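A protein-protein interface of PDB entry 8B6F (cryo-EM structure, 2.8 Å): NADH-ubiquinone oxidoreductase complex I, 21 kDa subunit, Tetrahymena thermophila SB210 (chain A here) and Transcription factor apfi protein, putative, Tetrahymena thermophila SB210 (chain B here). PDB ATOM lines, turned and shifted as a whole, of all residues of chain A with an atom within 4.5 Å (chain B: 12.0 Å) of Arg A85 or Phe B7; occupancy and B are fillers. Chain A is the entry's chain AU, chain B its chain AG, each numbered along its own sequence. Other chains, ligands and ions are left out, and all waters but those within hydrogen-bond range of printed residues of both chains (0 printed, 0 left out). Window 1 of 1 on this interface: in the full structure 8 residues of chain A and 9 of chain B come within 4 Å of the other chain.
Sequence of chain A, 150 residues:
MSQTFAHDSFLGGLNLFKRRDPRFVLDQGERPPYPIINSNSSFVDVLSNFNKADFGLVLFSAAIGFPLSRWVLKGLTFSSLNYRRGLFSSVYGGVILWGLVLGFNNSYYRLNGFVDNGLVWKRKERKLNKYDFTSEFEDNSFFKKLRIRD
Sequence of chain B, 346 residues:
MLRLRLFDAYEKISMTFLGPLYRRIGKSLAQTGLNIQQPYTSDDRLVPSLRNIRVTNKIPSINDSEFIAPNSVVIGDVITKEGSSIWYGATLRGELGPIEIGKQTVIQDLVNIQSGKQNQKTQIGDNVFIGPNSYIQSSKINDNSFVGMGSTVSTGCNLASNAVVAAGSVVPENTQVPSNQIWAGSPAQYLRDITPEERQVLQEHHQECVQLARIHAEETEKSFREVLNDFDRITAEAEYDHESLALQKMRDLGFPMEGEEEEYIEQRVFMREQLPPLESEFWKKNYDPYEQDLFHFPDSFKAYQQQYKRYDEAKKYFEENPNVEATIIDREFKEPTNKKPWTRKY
Of the printed residues of chain B, Arg A85 touches Leu B4, Phe B7 and Asp B8. Of chain A, only Phe A66, Arg A85 and Phe A88 come within 4 Å of Phe B7. No residue of chain B comes within 4 Å of Asn A82. No residue of chain B comes within 4 Å of Arg A84. No residue of chain B comes within 4 Å of Leu A87. Printed residues of chain B within 4 Å of Phe A88: Phe B7 (3.7 Å). Printed residues of chain B within 4 Å of Ser A89: Arg B3. Of the printed residues of chain A, Leu B6 touches Phe A66. Of the printed residues of chain A, Arg B3 touches Ser A89 (3.1 Å). Thr B16 touches none of the printed residues of chain A. The nearest printed residue of chain A that does not touch Asp B8 is Phe A66 (5.8 Å).
The backbone carbonyl oxygen (O) of Leu B4 lies close to the side-chain carboxylate (OD1) of Asp B8. O of Tyr B10 sits at hydrogen-bond distance from OG of Ser B14 (3.2 Å).
Of the 17 printed residues of chain B, 6 touch a printed residue of chain A. Hydrophobic or aromatic side chains of chain B within 4 Å of the printed part of chain A: Leu B4, Phe B7 and Tyr B10. Of the 10 printed residues of chain A, 4 touch a printed residue of chain B. Among the printed residues, Asp or Glu carboxylates within 4 Å of a Lys or Arg side-chain nitrogen of the other chain: Arg A85 with Asp B8 (3.6 Å).
Among the printed residues, pairs that only touch across the chains: Phe A66 with Tyr B10 (3.3 Å), Arg A85 with Leu B4 (3.6 Å), Phe A88 with Phe B7 (3.7 Å), Phe A66 with Leu B6 (3.7 Å), Phe A66 with Phe B7 (3.8 Å) and Arg A85 with Phe B7 (3.9 Å).
The guanidinium group (NH2) of Arg B3 sits at hydrogen-bond distance from the side-chain hydroxyl (OG) of Ser A89 (3.1 Å). OD1 of Asp B8 is in salt-bridge range of NH2 of Arg A85.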
ATOM      1  N   PHE A  66      -9.200 -33.695  33.789  1.00  0.00           N
ATOM      2  CA  PHE A  66      -9.450 -32.748  32.713  1.00  0.00           C
ATOM      3  C   PHE A  66     -10.517 -31.752  33.154  1.00  0.00           C
ATOM      4  O   PHE A  66     -10.283 -30.538  33.091  1.00  0.00           O
ATOM      5  CB  PHE A  66      -9.859 -33.470  31.427  1.00  0.00           C
ATOM      6  CG  PHE A  66      -9.669 -32.647  30.191  1.00  0.00           C
ATOM      7  CD1 PHE A  66     -10.644 -31.756  29.781  1.00  0.00           C
ATOM      8  CD2 PHE A  66      -8.514 -32.763  29.439  1.00  0.00           C
ATOM      9  CE1 PHE A  66     -10.471 -30.997  28.644  1.00  0.00           C
ATOM     10  CE2 PHE A  66      -8.334 -32.007  28.301  1.00  0.00           C
ATOM     11  CZ  PHE A  66      -9.315 -31.121  27.903  1.00  0.00           C
ATOM     12  N   LEU A  81      -1.637 -17.327  26.133  1.00  0.00           N
ATOM     13  CA  LEU A  81      -2.021 -18.686  25.770  1.00  0.00           C
ATOM     14  C   LEU A  81      -0.974 -19.690  26.233  1.00  0.00           C
ATOM     15  O   LEU A  81      -1.313 -20.784  26.695  1.00  0.00           O
ATOM     16  CB  LEU A  81      -2.232 -18.790  24.258  1.00  0.00           C
ATOM     17  CG  LEU A  81      -2.703 -20.149  23.734  1.00  0.00           C
ATOM     18  CD1 LEU A  81      -4.071 -20.503  24.288  1.00  0.00           C
ATOM     19  CD2 LEU A  81      -2.728 -20.160  22.218  1.00  0.00           C
ATOM     20  N   ASN A  82       0.305 -19.339  26.108  1.00  0.00           N
ATOM     21  CA  ASN A  82       1.364 -20.250  26.527  1.00  0.00           C
ATOM     22  C   ASN A  82       1.288 -20.526  28.023  1.00  0.00           C
ATOM     23  O   ASN A  82       1.410 -21.675  28.461  1.00  0.00           O
ATOM     24  CB  ASN A  82       2.727 -19.669  26.154  1.00  0.00           C
ATOM     25  CG  ASN A  82       3.855 -20.652  26.368  1.00  0.00           C
ATOM     26  OD1 ASN A  82       3.650 -21.864  26.341  1.00  0.00           O
ATOM     27  ND2 ASN A  82       5.058 -20.135  26.584  1.00  0.00           N
ATOM     28  N   TYR A  83       1.102 -19.479  28.829  1.00  0.00           N
ATOM     29  CA  TYR A  83       1.017 -19.679  30.271  1.00  0.00           C
ATOM     30  C   TYR A  83      -0.242 -20.443  30.655  1.00  0.00           C
ATOM     31  O   TYR A  83      -0.216 -21.267  31.575  1.00  0.00           O
ATOM     32  CB  TYR A  83       1.061 -18.338  31.001  1.00  0.00           C
ATOM     33  CG  TYR A  83       0.931 -18.488  32.497  1.00  0.00           C
ATOM     34  CD1 TYR A  83       1.926 -19.107  33.239  1.00  0.00           C
ATOM     35  CD2 TYR A  83      -0.187 -18.015  33.165  1.00  0.00           C
ATOM     36  CE1 TYR A  83       1.811 -19.250  34.605  1.00  0.00           C
ATOM     37  CE2 TYR A  83      -0.312 -18.154  34.532  1.00  0.00           C
ATOM     38  CZ  TYR A  83       0.691 -18.773  35.246  1.00  0.00           C
ATOM     39  OH  TYR A  83       0.572 -18.912  36.607  1.00  0.00           O
ATOM     40  N   ARG A  84      -1.357 -20.178  29.972  1.00  0.00           N
ATOM     41  CA  ARG A  84      -2.584 -20.912  30.262  1.00  0.00           C
ATOM     42  C   ARG A  84      -2.412 -22.396  29.970  1.00  0.00           C
ATOM     43  O   ARG A  84      -2.828 -23.247  30.764  1.00  0.00           O
ATOM     44  CB  ARG A  84      -3.742 -20.335  29.450  1.00  0.00           C
ATOM     45  CG  ARG A  84      -5.087 -20.969  29.756  1.00  0.00           C
ATOM     46  CD  ARG A  84      -6.184 -20.361  28.900  1.00  0.00           C
ATOM     47  NE  ARG A  84      -6.339 -18.932  29.142  1.00  0.00           N
ATOM     48  CZ  ARG A  84      -7.124 -18.404  30.072  1.00  0.00           C
ATOM     49  NH1 ARG A  84      -7.845 -19.162  30.882  1.00  0.00           N
ATOM     50  NH2 ARG A  84      -7.188 -17.082  30.191  1.00  0.00           N
ATOM     51  N   ARG A  85      -1.813 -22.727  28.825  1.00  0.00           N
ATOM     52  CA  ARG A  85      -1.583 -24.128  28.491  1.00  0.00           C
ATOM     53  C   ARG A  85      -0.608 -24.769  29.469  1.00  0.00           C
ATOM     54  O   ARG A  85      -0.785 -25.926  29.865  1.00  0.00           O
ATOM     55  CB  ARG A  85      -1.077 -24.242  27.053  1.00  0.00           C
ATOM     56  CG  ARG A  85      -2.114 -23.801  26.028  1.00  0.00           C
ATOM     57  CD  ARG A  85      -1.527 -23.599  24.639  1.00  0.00           C
ATOM     58  NE  ARG A  85      -1.327 -24.851  23.918  1.00  0.00           N
ATOM     59  CZ  ARG A  85      -0.157 -25.453  23.745  1.00  0.00           C
ATOM     60  NH1 ARG A  85       0.963 -24.955  24.245  1.00  0.00           N
ATOM     61  NH2 ARG A  85      -0.109 -26.585  23.050  1.00  0.00           N
ATOM     62  N   GLY A  86       0.426 -24.032  29.871  1.00  0.00           N
ATOM     63  CA  GLY A  86       1.359 -24.560  30.853  1.00  0.00           C
ATOM     64  C   GLY A  86       0.704 -24.824  32.195  1.00  0.00           C
ATOM     65  O   GLY A  86       0.970 -25.843  32.836  1.00  0.00           O
ATOM     66  N   LEU A  87      -0.164 -23.912  32.635  1.00  0.00           N
ATOM     67  CA  LEU A  87      -0.872 -24.113  33.894  1.00  0.00           C
ATOM     68  C   LEU A  87      -1.801 -25.316  33.815  1.00  0.00           C
ATOM     69  O   LEU A  87      -1.891 -26.103  34.764  1.00  0.00           O
ATOM     70  CB  LEU A  87      -1.651 -22.852  34.263  1.00  0.00           C
ATOM     71  CG  LEU A  87      -2.454 -22.908  35.565  1.00  0.00           C
ATOM     72  CD1 LEU A  87      -1.555 -23.168  36.763  1.00  0.00           C
ATOM     73  CD2 LEU A  87      -3.229 -21.619  35.755  1.00  0.00           C
ATOM     74  N   PHE A  88      -2.503 -25.477  32.692  1.00  0.00           N
ATOM     75  CA  PHE A  88      -3.338 -26.659  32.510  1.00  0.00           C
ATOM     76  C   PHE A  88      -2.501 -27.927  32.582  1.00  0.00           C
ATOM     77  O   PHE A  88      -2.892 -28.904  33.230  1.00  0.00           O
ATOM     78  CB  PHE A  88      -4.077 -26.587  31.174  1.00  0.00           C
ATOM     79  CG  PHE A  88      -4.944 -27.780  30.901  1.00  0.00           C
ATOM     80  CD1 PHE A  88      -4.430 -28.900  30.270  1.00  0.00           C
ATOM     81  CD2 PHE A  88      -6.275 -27.783  31.280  1.00  0.00           C
ATOM     82  CE1 PHE A  88      -5.225 -29.999  30.023  1.00  0.00           C
ATOM     83  CE2 PHE A  88      -7.077 -28.879  31.036  1.00  0.00           C
ATOM     84  CZ  PHE A  88      -6.551 -29.988  30.407  1.00  0.00           C
ATOM     85  N   SER A  89      -1.345 -27.930  31.919  1.00  0.00           N
ATOM     86  CA  SER A  89      -0.476 -29.099  31.957  1.00  0.00           C
ATOM     87  C   SER A  89      -0.020 -29.394  33.379  1.00  0.00           C
ATOM     88  O   SER A  89       0.010 -30.556  33.800  1.00  0.00           O
ATOM     89  CB  SER A  89       0.726 -28.877  31.039  1.00  0.00           C
ATOM     90  OG  SER A  89       1.649 -29.948  31.134  1.00  0.00           O
ATOM     91  N   MET B   1       2.875 -33.366  25.645  1.00  0.00           N
ATOM     92  CA  MET B   1       2.408 -33.927  24.346  1.00  0.00           C
ATOM     93  C   MET B   1       0.950 -34.354  24.440  1.00  0.00           C
ATOM     94  O   MET B   1       0.064 -33.688  23.908  1.00  0.00           O
ATOM     95  CB  MET B   1       3.273 -35.119  23.930  1.00  0.00           C
ATOM     96  CG  MET B   1       4.704 -34.755  23.573  1.00  0.00           C
ATOM     97  SD  MET B   1       5.668 -36.180  23.034  1.00  0.00           S
ATOM     98  CE  MET B   1       7.249 -35.416  22.689  1.00  0.00           C
ATOM     99  N   LEU B   2       0.709 -35.475  25.120  1.00  0.00           N
ATOM    100  CA  LEU B   2      -0.649 -36.003  25.209  1.00  0.00           C
ATOM    101  C   LEU B   2      -1.575 -35.027  25.919  1.00  0.00           C
ATOM    102  O   LEU B   2      -2.705 -34.795  25.473  1.00  0.00           O
ATOM    103  CB  LEU B   2      -0.639 -37.349  25.932  1.00  0.00           C
ATOM    104  CG  LEU B   2       0.272 -38.424  25.335  1.00  0.00           C
ATOM    105  CD1 LEU B   2       0.264 -39.666  26.209  1.00  0.00           C
ATOM    106  CD2 LEU B   2      -0.145 -38.763  23.914  1.00  0.00           C
ATOM    107  N   ARG B   3      -1.112 -34.435  27.020  1.00  0.00           N
ATOM    108  CA  ARG B   3      -1.970 -33.546  27.797  1.00  0.00           C
ATOM    109  C   ARG B   3      -2.374 -32.324  26.982  1.00  0.00           C
ATOM    110  O   ARG B   3      -3.556 -31.970  26.917  1.00  0.00           O
ATOM    111  CB  ARG B   3      -1.258 -33.132  29.084  1.00  0.00           C
ATOM    112  CG  ARG B   3      -0.835 -34.314  29.945  1.00  0.00           C
ATOM    113  CD  ARG B   3      -0.124 -33.869  31.209  1.00  0.00           C
ATOM    114  NE  ARG B   3       1.211 -33.360  30.924  1.00  0.00           N
ATOM    115  CZ  ARG B   3       2.096 -33.013  31.848  1.00  0.00           C
ATOM    116  NH1 ARG B   3       1.820 -33.105  33.138  1.00  0.00           N
ATOM    117  NH2 ARG B   3       3.288 -32.564  31.469  1.00  0.00           N
ATOM    118  N   LEU B   4      -1.401 -31.663  26.352  1.00  0.00           N
ATOM    119  CA  LEU B   4      -1.712 -30.475  25.566  1.00  0.00           C
ATOM    120  C   LEU B   4      -2.537 -30.822  24.334  1.00  0.00           C
ATOM    121  O   LEU B   4      -3.418 -30.051  23.934  1.00  0.00           O
ATOM    122  CB  LEU B   4      -0.424 -29.756  25.167  1.00  0.00           C
ATOM    123  CG  LEU B   4       0.305 -29.004  26.282  1.00  0.00           C
ATOM    124  CD1 LEU B   4       1.608 -28.419  25.770  1.00  0.00           C
ATOM    125  CD2 LEU B   4      -0.569 -27.906  26.866  1.00  0.00           C
ATOM    126  N   ARG B   5      -2.276 -31.977  23.719  1.00  0.00           N
ATOM    127  CA  ARG B   5      -3.069 -32.380  22.562  1.00  0.00           C
ATOM    128  C   ARG B   5      -4.519 -32.628  22.955  1.00  0.00           C
ATOM    129  O   ARG B   5      -5.439 -32.242  22.226  1.00  0.00           O
ATOM    130  CB  ARG B   5      -2.461 -33.617  21.908  1.00  0.00           C
ATOM    131  CG  ARG B   5      -1.282 -33.293  21.006  1.00  0.00           C
ATOM    132  CD  ARG B   5      -0.735 -34.527  20.317  1.00  0.00           C
ATOM    133  NE  ARG B   5       0.273 -34.180  19.323  1.00  0.00           N
ATOM    134  CZ  ARG B   5       1.535 -33.890  19.605  1.00  0.00           C
ATOM    135  NH1 ARG B   5       1.987 -33.896  20.848  1.00  0.00           N
ATOM    136  NH2 ARG B   5       2.367 -33.586  18.613  1.00  0.00           N
ATOM    137  N   LEU B   6      -4.744 -33.276  24.098  1.00  0.00           N
ATOM    138  CA  LEU B   6      -6.107 -33.435  24.590  1.00  0.00           C
ATOM    139  C   LEU B   6      -6.746 -32.081  24.871  1.00  0.00           C
ATOM    140  O   LEU B   6      -7.926 -31.868  24.569  1.00  0.00           O
ATOM    141  CB  LEU B   6      -6.116 -34.302  25.849  1.00  0.00           C
ATOM    142  CG  LEU B   6      -6.410 -35.790  25.638  1.00  0.00           C
ATOM    143  CD1 LEU B   6      -5.415 -36.426  24.681  1.00  0.00           C
ATOM    144  CD2 LEU B   6      -6.401 -36.514  26.972  1.00  0.00           C
ATOM    145  N   PHE B   7      -5.985 -31.156  25.457  1.00  0.00           N
ATOM    146  CA  PHE B   7      -6.521 -29.829  25.742  1.00  0.00           C
ATOM    147  C   PHE B   7      -6.957 -29.129  24.462  1.00  0.00           C
ATOM    148  O   PHE B   7      -8.054 -28.566  24.389  1.00  0.00           O
ATOM    149  CB  PHE B   7      -5.477 -28.994  26.483  1.00  0.00           C
ATOM    150  CG  PHE B   7      -5.904 -27.577  26.740  1.00  0.00           C
ATOM    151  CD1 PHE B   7      -6.854 -27.294  27.706  1.00  0.00           C
ATOM    152  CD2 PHE B   7      -5.347 -26.529  26.026  1.00  0.00           C
ATOM    153  CE1 PHE B   7      -7.248 -25.994  27.950  1.00  0.00           C
ATOM    154  CE2 PHE B   7      -5.736 -25.224  26.266  1.00  0.00           C
ATOM    155  CZ  PHE B   7      -6.688 -24.956  27.230  1.00  0.00           C
ATOM    156  N   ASP B   8      -6.104 -29.151  23.437  1.00  0.00           N
ATOM    157  CA  ASP B   8      -6.442 -28.488  22.182  1.00  0.00           C
ATOM    158  C   ASP B   8      -7.619 -29.169  21.496  1.00  0.00           C
ATOM    159  O   ASP B   8      -8.502 -28.498  20.950  1.00  0.00           O
ATOM    160  CB  ASP B   8      -5.227 -28.459  21.257  1.00  0.00           C
ATOM    161  CG  ASP B   8      -4.166 -27.485  21.724  1.00  0.00           C
ATOM    162  OD1 ASP B   8      -3.476 -27.785  22.720  1.00  0.00           O
ATOM    163  OD2 ASP B   8      -4.026 -26.414  21.098  1.00  0.00           O
ATOM    164  N   ALA B   9      -7.646 -30.502  21.507  1.00  0.00           N
ATOM    165  CA  ALA B   9      -8.762 -31.218  20.900  1.00  0.00           C
ATOM    166  C   ALA B   9     -10.074 -30.873  21.588  1.00  0.00           C
ATOM    167  O   ALA B   9     -11.091 -30.645  20.923  1.00  0.00           O
ATOM    168  CB  ALA B   9      -8.509 -32.724  20.952  1.00  0.00           C
ATOM    169  N   TYR B  10     -10.075 -30.828  22.922  1.00  0.00           N
ATOM    170  CA  TYR B  10     -11.293 -30.479  23.642  1.00  0.00           C
ATOM    171  C   TYR B  10     -11.695 -29.033  23.381  1.00  0.00           C
ATOM    172  O   TYR B  10     -12.885 -28.731  23.245  1.00  0.00           O
ATOM    173  CB  TYR B  10     -11.118 -30.714  25.141  1.00  0.00           C
ATOM    174  CG  TYR B  10     -12.392 -30.479  25.920  1.00  0.00           C
ATOM    175  CD1 TYR B  10     -12.738 -29.207  26.361  1.00  0.00           C
ATOM    176  CD2 TYR B  10     -13.254 -31.529  26.203  1.00  0.00           C
ATOM    177  CE1 TYR B  10     -13.905 -28.989  27.066  1.00  0.00           C
ATOM    178  CE2 TYR B  10     -14.424 -31.322  26.907  1.00  0.00           C
ATOM    179  CZ  TYR B  10     -14.743 -30.051  27.336  1.00  0.00           C
ATOM    180  OH  TYR B  10     -15.906 -29.842  28.040  1.00  0.00           O
ATOM    181  N   GLU B  11     -10.721 -28.122  23.313  1.00  0.00           N
ATOM    182  CA  GLU B  11     -11.044 -26.732  23.013  1.00  0.00           C
ATOM    183  C   GLU B  11     -11.740 -26.620  21.663  1.00  0.00           C
ATOM    184  O   GLU B  11     -12.778 -25.962  21.540  1.00  0.00           O
ATOM    185  CB  GLU B  11      -9.772 -25.882  23.034  1.00  0.00           C
ATOM    186  CG  GLU B  11      -9.208 -25.631  24.424  1.00  0.00           C
ATOM    187  CD  GLU B  11     -10.084 -24.713  25.256  1.00  0.00           C
ATOM    188  OE1 GLU B  11     -11.039 -24.134  24.700  1.00  0.00           O
ATOM    189  OE2 GLU B  11      -9.817 -24.573  26.468  1.00  0.00           O
ATOM    190  N   LYS B  12     -11.174 -27.252  20.634  1.00  0.00           N
ATOM    191  CA  LYS B  12     -11.794 -27.201  19.315  1.00  0.00           C
ATOM    192  C   LYS B  12     -13.173 -27.848  19.334  1.00  0.00           C
ATOM    193  O   LYS B  12     -14.129 -27.306  18.768  1.00  0.00           O
ATOM    194  CB  LYS B  12     -10.893 -27.882  18.285  1.00  0.00           C
ATOM    195  CG  LYS B  12      -9.649 -27.080  17.932  1.00  0.00           C
ATOM    196  CD  LYS B  12      -8.816 -27.784  16.871  1.00  0.00           C
ATOM    197  CE  LYS B  12      -7.657 -26.914  16.405  1.00  0.00           C
ATOM    198  NZ  LYS B  12      -6.752 -26.525  17.523  1.00  0.00           N
ATOM    199  N   ILE B  13     -13.296 -29.010  19.980  1.00  0.00           N
ATOM    200  CA  ILE B  13     -14.580 -29.709  20.009  1.00  0.00           C
ATOM    201  C   ILE B  13     -15.637 -28.848  20.686  1.00  0.00           C
ATOM    202  O   ILE B  13     -16.756 -28.698  20.181  1.00  0.00           O
ATOM    203  CB  ILE B  13     -14.431 -31.073  20.710  1.00  0.00           C
ATOM    204  CG1 ILE B  13     -13.645 -32.039  19.820  1.00  0.00           C
ATOM    205  CG2 ILE B  13     -15.799 -31.665  21.054  1.00  0.00           C
ATOM    206  CD1 ILE B  13     -13.239 -33.328  20.514  1.00  0.00           C
ATOM    207  N   SER B  14     -15.305 -28.273  21.843  1.00  0.00           N
ATOM    208  CA  SER B  14     -16.264 -27.418  22.533  1.00  0.00           C
ATOM    209  C   SER B  14     -16.671 -26.244  21.652  1.00  0.00           C
ATOM    210  O   SER B  14     -17.862 -26.006  21.423  1.00  0.00           O
ATOM    211  CB  SER B  14     -15.677 -26.926  23.857  1.00  0.00           C
ATOM    212  OG  SER B  14     -14.558 -26.087  23.642  1.00  0.00           O
ATOM    213  N   MET B  15     -15.687 -25.488  21.162  1.00  0.00           N
ATOM    214  CA  MET B  15     -15.989 -24.279  20.404  1.00  0.00           C
ATOM    215  C   MET B  15     -16.801 -24.576  19.150  1.00  0.00           C
ATOM    216  O   MET B  15     -17.624 -23.751  18.739  1.00  0.00           O
ATOM    217  CB  MET B  15     -14.685 -23.576  20.030  1.00  0.00           C
ATOM    218  CG  MET B  15     -14.870 -22.232  19.344  1.00  0.00           C
ATOM    219  SD  MET B  15     -13.310 -21.492  18.819  1.00  0.00           S
ATOM    220  CE  MET B  15     -12.428 -21.393  20.373  1.00  0.00           C
ATOM    221  N   THR B  16     -16.590 -25.739  18.527  1.00  0.00           N
ATOM    222  CA  THR B  16     -17.231 -26.033  17.251  1.00  0.00           C
ATOM    223  C   THR B  16     -18.531 -26.813  17.388  1.00  0.00           C
ATOM    224  O   THR B  16     -19.342 -26.798  16.455  1.00  0.00           O
ATOM    225  CB  THR B  16     -16.264 -26.816  16.351  1.00  0.00           C
ATOM    226  OG1 THR B  16     -15.057 -26.065  16.172  1.00  0.00           O
ATOM    227  CG2 THR B  16     -16.881 -27.089  14.980  1.00  0.00           C
ATOM    228  N   LEU B  18     -20.299 -27.583  21.010  1.00  0.00           N
ATOM    229  CA  LEU B  18     -21.147 -27.249  22.149  1.00  0.00           C
ATOM    230  C   LEU B  18     -21.672 -25.825  22.047  1.00  0.00           C
ATOM    231  O   LEU B  18     -22.831 -25.560  22.386  1.00  0.00           O
ATOM    232  CB  LEU B  18     -20.377 -27.444  23.454  1.00  0.00           C
ATOM    233  CG  LEU B  18     -19.849 -28.856  23.712  1.00  0.00           C
ATOM    234  CD1 LEU B  18     -19.060 -28.894  25.006  1.00  0.00           C
ATOM    235  CD2 LEU B  18     -20.980 -29.870  23.746  1.00  0.00           C
